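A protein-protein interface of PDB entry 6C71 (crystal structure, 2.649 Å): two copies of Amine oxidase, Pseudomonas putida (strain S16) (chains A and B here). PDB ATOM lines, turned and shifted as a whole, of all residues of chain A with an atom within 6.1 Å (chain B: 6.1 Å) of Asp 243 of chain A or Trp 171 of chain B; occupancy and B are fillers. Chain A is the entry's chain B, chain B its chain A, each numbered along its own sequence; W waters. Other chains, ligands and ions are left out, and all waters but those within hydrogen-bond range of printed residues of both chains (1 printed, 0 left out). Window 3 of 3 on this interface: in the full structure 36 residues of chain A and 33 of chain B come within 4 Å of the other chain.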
ATOM      1  N   ARG A 160      22.734  10.190  24.495  1.00  0.00           N
ATOM      2  CA  ARG A 160      22.419   9.117  23.557  1.00  0.00           C
ATOM      3  C   ARG A 160      21.731   7.962  24.272  1.00  0.00           C
ATOM      4  O   ARG A 160      20.682   7.476  23.831  1.00  0.00           O
ATOM      5  CB  ARG A 160      23.698   8.621  22.886  1.00  0.00           C
ATOM      6  CG  ARG A 160      23.481   7.699  21.698  1.00  0.00           C
ATOM      7  CD  ARG A 160      24.635   6.715  21.558  1.00  0.00           C
ATOM      8  NE  ARG A 160      25.951   7.351  21.581  1.00  0.00           N
ATOM      9  CZ  ARG A 160      26.425   8.184  20.660  1.00  0.00           C
ATOM     10  NH1 ARG A 160      25.699   8.510  19.600  1.00  0.00           N
ATOM     11  NH2 ARG A 160      27.642   8.694  20.805  1.00  0.00           N
ATOM     12  N   GLU A 164      17.826   6.931  23.658  1.00  0.00           N
ATOM     13  CA  GLU A 164      17.553   5.643  23.031  1.00  0.00           C
ATOM     14  C   GLU A 164      16.789   4.712  23.967  1.00  0.00           C
ATOM     15  O   GLU A 164      15.996   3.886  23.499  1.00  0.00           O
ATOM     16  CB  GLU A 164      18.861   5.006  22.559  1.00  0.00           C
ATOM     17  CG  GLU A 164      19.528   5.787  21.433  1.00  0.00           C
ATOM     18  CD  GLU A 164      20.506   4.957  20.625  1.00  0.00           C
ATOM     19  OE1 GLU A 164      21.343   4.254  21.236  1.00  0.00           O
ATOM     20  OE2 GLU A 164      20.452   5.024  19.382  1.00  0.00           O
ATOM     21  N   PHE A 235      10.986  10.621  16.727  1.00  0.00           N
ATOM     22  CA  PHE A 235      12.203   9.817  16.694  1.00  0.00           C
ATOM     23  C   PHE A 235      12.167   8.808  15.552  1.00  0.00           C
ATOM     24  O   PHE A 235      13.186   8.567  14.893  1.00  0.00           O
ATOM     25  CB  PHE A 235      12.400   9.108  18.034  1.00  0.00           C
ATOM     26  CG  PHE A 235      13.644   8.270  18.102  1.00  0.00           C
ATOM     27  CD1 PHE A 235      13.577   6.896  17.943  1.00  0.00           C
ATOM     28  CD2 PHE A 235      14.877   8.851  18.336  1.00  0.00           C
ATOM     29  CE1 PHE A 235      14.716   6.119  18.011  1.00  0.00           C
ATOM     30  CE2 PHE A 235      16.021   8.079  18.403  1.00  0.00           C
ATOM     31  CZ  PHE A 235      15.940   6.712  18.240  1.00  0.00           C
ATOM     32  N   ASN A 241      16.926   6.436  14.874  1.00  0.00           N
ATOM     33  CA  ASN A 241      18.312   6.472  15.315  1.00  0.00           C
ATOM     34  C   ASN A 241      18.604   7.858  15.869  1.00  0.00           C
ATOM     35  O   ASN A 241      18.299   8.863  15.220  1.00  0.00           O
ATOM     36  CB  ASN A 241      19.248   6.116  14.149  1.00  0.00           C
ATOM     37  CG  ASN A 241      20.649   6.659  14.325  1.00  0.00           C
ATOM     38  OD1 ASN A 241      20.941   7.792  13.948  1.00  0.00           O
ATOM     39  ND2 ASN A 241      21.535   5.837  14.879  1.00  0.00           N
ATOM     40  N   TYR A 242      19.198   7.908  17.066  1.00  0.00           N
ATOM     41  CA  TYR A 242      19.329   9.182  17.768  1.00  0.00           C
ATOM     42  C   TYR A 242      20.303  10.122  17.071  1.00  0.00           C
ATOM     43  O   TYR A 242      20.111  11.341  17.097  1.00  0.00           O
ATOM     44  CB  TYR A 242      19.759   8.969  19.218  1.00  0.00           C
ATOM     45  CG  TYR A 242      20.269  10.247  19.850  1.00  0.00           C
ATOM     46  CD1 TYR A 242      19.393  11.270  20.195  1.00  0.00           C
ATOM     47  CD2 TYR A 242      21.625  10.439  20.082  1.00  0.00           C
ATOM     48  CE1 TYR A 242      19.852  12.445  20.760  1.00  0.00           C
ATOM     49  CE2 TYR A 242      22.093  11.611  20.649  1.00  0.00           C
ATOM     50  CZ  TYR A 242      21.203  12.609  20.986  1.00  0.00           C
ATOM     51  OH  TYR A 242      21.667  13.775  21.551  1.00  0.00           O
ATOM     52  N   ASP A 243      21.372   9.591  16.480  1.00  0.00           N
ATOM     53  CA  ASP A 243      22.354  10.460  15.836  1.00  0.00           C
ATOM     54  C   ASP A 243      21.720  11.241  14.689  1.00  0.00           C
ATOM     55  O   ASP A 243      21.833  12.472  14.619  1.00  0.00           O
ATOM     56  CB  ASP A 243      23.544   9.631  15.352  1.00  0.00           C
ATOM     57  CG  ASP A 243      24.439   9.181  16.492  1.00  0.00           C
ATOM     58  OD1 ASP A 243      24.615   9.959  17.453  1.00  0.00           O
ATOM     59  OD2 ASP A 243      24.965   8.050  16.430  1.00  0.00           O
ATOM     60  N   ALA A 244      21.028  10.538  13.790  1.00  0.00           N
ATOM     61  CA  ALA A 244      20.356  11.205  12.680  1.00  0.00           C
ATOM     62  C   ALA A 244      19.292  12.174  13.186  1.00  0.00           C
ATOM     63  O   ALA A 244      19.244  13.336  12.764  1.00  0.00           O
ATOM     64  CB  ALA A 244      19.741  10.166  11.742  1.00  0.00           C
ATOM     65  N   PHE A 245      18.436  11.713  14.104  1.00  0.00           N
ATOM     66  CA  PHE A 245      17.367  12.566  14.615  1.00  0.00           C
ATOM     67  C   PHE A 245      17.926  13.840  15.234  1.00  0.00           C
ATOM     68  O   PHE A 245      17.384  14.931  15.026  1.00  0.00           O
ATOM     69  CB  PHE A 245      16.521  11.810  15.639  1.00  0.00           C
ATOM     70  CG  PHE A 245      15.499  12.673  16.322  1.00  0.00           C
ATOM     71  CD1 PHE A 245      15.724  13.167  17.598  1.00  0.00           C
ATOM     72  CD2 PHE A 245      14.319  13.006  15.678  1.00  0.00           C
ATOM     73  CE1 PHE A 245      14.786  13.970  18.221  1.00  0.00           C
ATOM     74  CE2 PHE A 245      13.378  13.808  16.295  1.00  0.00           C
ATOM     75  CZ  PHE A 245      13.611  14.290  17.568  1.00  0.00           C
ATOM     76  N   MET A 246      19.002  13.715  16.009  1.00  0.00           N
ATOM     77  CA  MET A 246      19.635  14.886  16.600  1.00  0.00           C
ATOM     78  C   MET A 246      20.192  15.795  15.514  1.00  0.00           C
ATOM     79  O   MET A 246      20.134  17.025  15.630  1.00  0.00           O
ATOM     80  CB  MET A 246      20.750  14.447  17.551  1.00  0.00           C
ATOM     81  CG  MET A 246      21.452  15.570  18.308  1.00  0.00           C
ATOM     82  SD  MET A 246      20.395  16.347  19.555  1.00  0.00           S
ATOM     83  CE  MET A 246      19.745  17.770  18.687  1.00  0.00           C
ATOM     84  N   ASP A 247      20.728  15.205  14.441  1.00  0.00           N
ATOM     85  CA  ASP A 247      21.203  16.009  13.319  1.00  0.00           C
ATOM     86  C   ASP A 247      20.069  16.771  12.644  1.00  0.00           C
ATOM     87  O   ASP A 247      20.299  17.846  12.076  1.00  0.00           O
ATOM     88  CB  ASP A 247      21.923  15.126  12.302  1.00  0.00           C
ATOM     89  CG  ASP A 247      22.966  15.887  11.506  1.00  0.00           C
ATOM     90  OD1 ASP A 247      23.649  16.754  12.093  1.00  0.00           O
ATOM     91  OD2 ASP A 247      23.101  15.623  10.293  1.00  0.00           O
ATOM     92  N   THR A 248      18.843  16.244  12.693  1.00  0.00           N
ATOM     93  CA  THR A 248      17.735  16.893  11.998  1.00  0.00           C
ATOM     94  C   THR A 248      17.229  18.148  12.699  1.00  0.00           C
ATOM     95  O   THR A 248      16.577  18.975  12.056  1.00  0.00           O
ATOM     96  CB  THR A 248      16.562  15.925  11.819  1.00  0.00           C
ATOM     97  OG1 THR A 248      16.010  15.589  13.100  1.00  0.00           O
ATOM     98  CG2 THR A 248      16.998  14.664  11.091  1.00  0.00           C
ATOM     99  N   CYS B 167      30.439   0.299   6.147  1.00  0.00           N
ATOM    100  CA  CYS B 167      30.168   1.733   6.145  1.00  0.00           C
ATOM    101  C   CYS B 167      30.545   2.379   7.475  1.00  0.00           C
ATOM    102  O   CYS B 167      29.858   3.280   7.960  1.00  0.00           O
ATOM    103  CB  CYS B 167      28.702   1.998   5.816  1.00  0.00           C
ATOM    104  SG  CYS B 167      28.165   1.319   4.227  1.00  0.00           S
ATOM    105  N   HIS B 168      31.645   1.920   8.079  1.00  0.00           N
ATOM    106  CA  HIS B 168      32.008   2.386   9.415  1.00  0.00           C
ATOM    107  C   HIS B 168      32.322   3.876   9.437  1.00  0.00           C
ATOM    108  O   HIS B 168      32.120   4.535  10.464  1.00  0.00           O
ATOM    109  CB  HIS B 168      33.193   1.577   9.949  1.00  0.00           C
ATOM    110  CG  HIS B 168      34.464   1.789   9.188  1.00  0.00           C
ATOM    111  ND1 HIS B 168      34.792   1.054   8.068  1.00  0.00           N
ATOM    112  CD2 HIS B 168      35.493   2.645   9.391  1.00  0.00           C
ATOM    113  CE1 HIS B 168      35.965   1.453   7.611  1.00  0.00           C
ATOM    114  NE2 HIS B 168      36.413   2.417   8.396  1.00  0.00           N
ATOM    115  N   ASP B 169      32.818   4.428   8.328  1.00  0.00           N
ATOM    116  CA  ASP B 169      33.193   5.833   8.256  1.00  0.00           C
ATOM    117  C   ASP B 169      32.181   6.671   7.483  1.00  0.00           C
ATOM    118  O   ASP B 169      32.493   7.803   7.099  1.00  0.00           O
ATOM    119  CB  ASP B 169      34.584   5.981   7.639  1.00  0.00           C
ATOM    120  CG  ASP B 169      34.721   5.247   6.318  1.00  0.00           C
ATOM    121  OD1 ASP B 169      33.826   4.442   5.982  1.00  0.00           O
ATOM    122  OD2 ASP B 169      35.728   5.473   5.613  1.00  0.00           O
ATOM    123  N   ALA B 170      30.973   6.144   7.264  1.00  0.00           N
ATOM    124  CA  ALA B 170      29.983   6.862   6.465  1.00  0.00           C
ATOM    125  C   ALA B 170      29.658   8.220   7.086  1.00  0.00           C
ATOM    126  O   ALA B 170      29.424   9.198   6.368  1.00  0.00           O
ATOM    127  CB  ALA B 170      28.721   6.010   6.299  1.00  0.00           C
ATOM    128  N   TRP B 171      29.636   8.297   8.423  1.00  0.00           N
ATOM    129  CA  TRP B 171      29.331   9.554   9.109  1.00  0.00           C
ATOM    130  C   TRP B 171      30.374  10.647   8.815  1.00  0.00           C
ATOM    131  O   TRP B 171      30.010  11.776   8.480  1.00  0.00           O
ATOM    132  CB  TRP B 171      29.175   9.297  10.613  1.00  0.00           C
ATOM    133  CG  TRP B 171      27.754   9.411  11.201  1.00  0.00           C
ATOM    134  CD1 TRP B 171      26.976   8.387  11.667  1.00  0.00           C
ATOM    135  CD2 TRP B 171      26.989  10.616  11.415  1.00  0.00           C
ATOM    136  NE1 TRP B 171      25.788   8.876  12.157  1.00  0.00           N
ATOM    137  CE2 TRP B 171      25.768  10.236  12.011  1.00  0.00           C
ATOM    138  CE3 TRP B 171      27.216  11.973  11.157  1.00  0.00           C
ATOM    139  CZ2 TRP B 171      24.780  11.160  12.356  1.00  0.00           C
ATOM    140  CZ3 TRP B 171      26.225  12.892  11.501  1.00  0.00           C
ATOM    141  CH2 TRP B 171      25.025  12.477  12.092  1.00  0.00           C
ATOM    142  N   GLU B 172      31.671  10.312   8.855  1.00  0.00           N
ATOM    143  CA  GLU B 172      32.748  11.294   8.706  1.00  0.00           C
ATOM    144  C   GLU B 172      32.760  11.778   7.271  1.00  0.00           C
ATOM    145  O   GLU B 172      32.947  12.968   6.954  1.00  0.00           O
ATOM    146  CB  GLU B 172      34.091  10.605   8.678  1.00  0.00           C
ATOM    147  CG  GLU B 172      34.349   9.601   9.679  1.00  0.00           C
ATOM    148  CD  GLU B 172      35.784   9.415  10.029  1.00  0.00           C
ATOM    149  OE1 GLU B 172      36.594  10.356  10.163  1.00  0.00           O
ATOM    150  OE2 GLU B 172      36.118   8.213  10.007  1.00  0.00           O
ATOM    151  N   VAL B 173      32.672  10.768   6.409  1.00  0.00           N
ATOM    152  CA  VAL B 173      33.002  10.911   5.018  1.00  0.00           C
ATOM    153  C   VAL B 173      31.875  11.611   4.320  1.00  0.00           C
ATOM    154  O   VAL B 173      32.097  12.423   3.424  1.00  0.00           O
ATOM    155  CB  VAL B 173      33.315   9.526   4.416  1.00  0.00           C
ATOM    156  CG1 VAL B 173      33.574   9.693   2.941  1.00  0.00           C
ATOM    157  CG2 VAL B 173      34.548   8.899   5.072  1.00  0.00           C
ATOM    158  N   PHE B 174      30.651  11.331   4.741  1.00  0.00           N
ATOM    159  CA  PHE B 174      29.462  11.936   4.158  1.00  0.00           C
ATOM    160  C   PHE B 174      28.592  12.513   5.264  1.00  0.00           C
ATOM    161  O   PHE B 174      27.521  11.980   5.571  1.00  0.00           O
ATOM    162  CB  PHE B 174      28.700  10.914   3.316  1.00  0.00           C
ATOM    163  CG  PHE B 174      29.415  10.525   2.056  1.00  0.00           C
ATOM    164  CD1 PHE B 174      29.400  11.368   0.959  1.00  0.00           C
ATOM    165  CD2 PHE B 174      30.089   9.319   1.960  1.00  0.00           C
ATOM    166  CE1 PHE B 174      30.045  11.020  -0.209  1.00  0.00           C
ATOM    167  CE2 PHE B 174      30.738   8.966   0.791  1.00  0.00           C
ATOM    168  CZ  PHE B 174      30.716   9.818  -0.294  1.00  0.00           C
ATOM    169  N   PRO B 175      29.031  13.607   5.897  1.00  0.00           N
ATOM    170  CA  PRO B 175      28.121  14.309   6.809  1.00  0.00           C
ATOM    171  C   PRO B 175      26.968  14.963   6.073  1.00  0.00           C
ATOM    172  O   PRO B 175      25.900  15.163   6.663  1.00  0.00           O
ATOM    173  CB  PRO B 175      29.029  15.347   7.486  1.00  0.00           C
ATOM    174  CG  PRO B 175      30.113  15.589   6.495  1.00  0.00           C
ATOM    175  CD  PRO B 175      30.343  14.273   5.809  1.00  0.00           C
ATOM    176  N   ARG B 176      27.156  15.298   4.795  1.00  0.00           N
ATOM    177  CA  ARG B 176      26.113  15.857   3.937  1.00  0.00           C
ATOM    178  C   ARG B 176      26.003  14.966   2.707  1.00  0.00           C
ATOM    179  O   ARG B 176      26.665  15.216   1.687  1.00  0.00           O
ATOM    180  CB  ARG B 176      26.432  17.296   3.543  1.00  0.00           C
ATOM    181  CG  ARG B 176      26.713  18.223   4.710  1.00  0.00           C
ATOM    182  CD  ARG B 176      26.862  19.652   4.223  1.00  0.00           C
ATOM    183  NE  ARG B 176      27.423  20.530   5.243  1.00  0.00           N
ATOM    184  CZ  ARG B 176      27.606  21.835   5.079  1.00  0.00           C
ATOM    185  NH1 ARG B 176      27.270  22.413   3.933  1.00  0.00           N
ATOM    186  NH2 ARG B 176      28.125  22.564   6.058  1.00  0.00           N
ATOM    187  N   ALA B 236      24.655   6.840   3.870  1.00  0.00           N
ATOM    188  CA  ALA B 236      24.476   8.107   4.571  1.00  0.00           C
ATOM    189  C   ALA B 236      23.103   8.715   4.309  1.00  0.00           C
ATOM    190  O   ALA B 236      22.533   9.361   5.196  1.00  0.00           O
ATOM    191  CB  ALA B 236      25.573   9.091   4.167  1.00  0.00           C
ATOM    192  N   GLY B 239      20.218   7.762   6.782  1.00  0.00           N
ATOM    193  CA  GLY B 239      20.392   8.052   8.191  1.00  0.00           C
ATOM    194  C   GLY B 239      21.595   7.419   8.851  1.00  0.00           C
ATOM    195  O   GLY B 239      21.612   7.295  10.080  1.00  0.00           O
ATOM    196  N   TRP B 240      22.599   7.003   8.074  1.00  0.00           N
ATOM    197  CA  TRP B 240      23.835   6.421   8.607  1.00  0.00           C
ATOM    198  C   TRP B 240      23.567   5.206   9.491  1.00  0.00           C
ATOM    199  O   TRP B 240      24.353   4.895  10.389  1.00  0.00           O
ATOM    200  CB  TRP B 240      24.655   7.451   9.389  1.00  0.00           C
ATOM    201  CG  TRP B 240      24.984   8.706   8.647  1.00  0.00           C
ATOM    202  CD1 TRP B 240      26.000   8.889   7.756  1.00  0.00           C
ATOM    203  CD2 TRP B 240      24.320   9.969   8.765  1.00  0.00           C
ATOM    204  NE1 TRP B 240      25.999  10.184   7.296  1.00  0.00           N
ATOM    205  CE2 TRP B 240      24.977  10.868   7.902  1.00  0.00           C
ATOM    206  CE3 TRP B 240      23.228  10.425   9.508  1.00  0.00           C
ATOM    207  CZ2 TRP B 240      24.579  12.196   7.763  1.00  0.00           C
ATOM    208  CZ3 TRP B 240      22.834  11.744   9.370  1.00  0.00           C
ATOM    209  CH2 TRP B 240      23.508  12.614   8.504  1.00  0.00           C
HETATM  210  O   HOH W   1      25.191  16.049   9.168  1.00  0.00           O
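The backbone carbonyl oxygen (O) of Phe 174 of chain B is in hydrogen-bond range of the indole nitrogen (NE1) of Trp 240 of chain B (2.9 Å).
The side-chain carboxylate (OD1) of Asp 243 of chain A is in salt-bridge range of the guanidinium group (NH1) of Arg 160 of chain A.
OD1 of Asn 241 of chain A is in hydrogen-bond range of N of Asp 243 of chain A (3.1 Å).
The side-chain amide oxygen (OD1) of Asn 241 of chain A is in hydrogen-bond range of the backbone NH (N) of Ala 244 of chain A (2.8 Å).
OD1 of Asn 241 of chain A touches O of Gly 239 of chain B (3.96 Å).
Asp 243 of chain A touches Trp 171 of chain B (CB to CZ2, 3.6 Å).
Ala 244 of chain A touches Gly 239 of chain B (CB to O, 3.8 Å).
OD2 of Asp 247 of chain A touches CH2 of Trp 240 of chain B, at 3.5 Å.
Of the printed residues of chain B, Asn 241 of chain A touches Gly 239.
Of the printed residues of chain B, Asp 243 of chain A touches Trp 171.
Of the printed residues of chain B, Ala 244 of chain A touches Gly 239.
Of chain A, only Asp 243 comes within 4 Å of Trp 171 of chain B.
Printed residues of chain A within 4 Å of Gly 239 of chain B: Asn 241 and Ala 244.
Of the printed residues of chain A, Trp 240 of chain B touches Asp 247 (3.5 Å).
The nearest residue of chain A that does not touch Trp 171 of chain B is Asp 247 of chain A (4.03 Å).
The nearest printed residue of chain B that does not touch Asp 247 of chain A is Trp 171 of chain B (4.03 Å).
Of the 11 printed residues of chain A, 4 touch a printed residue of chain B.
Hydrophobic or aromatic side chains of chain A that line the printed part of chain B: Ala 244.
Of the 13 printed residues of chain B, 3 touch a printed residue of chain A.
Among the printed residues, 4 pairs touch across the chains.
Among the printed residues, no Asp or Glu carboxylate lies within 4 Å of a Lys or Arg side-chain nitrogen of the other chain.
No position is printed for both chains.
Of the 4 pairs that touch across the chains among the printed residues, none has its exchanged pair printed and touching as well.
Water W1 lies within hydrogen-bond range of the side-chain carboxylate of Asp 247 of chain A (2.4 Å) and the backbone carbonyl oxygen of Pro 175 of chain B (2.8 Å).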
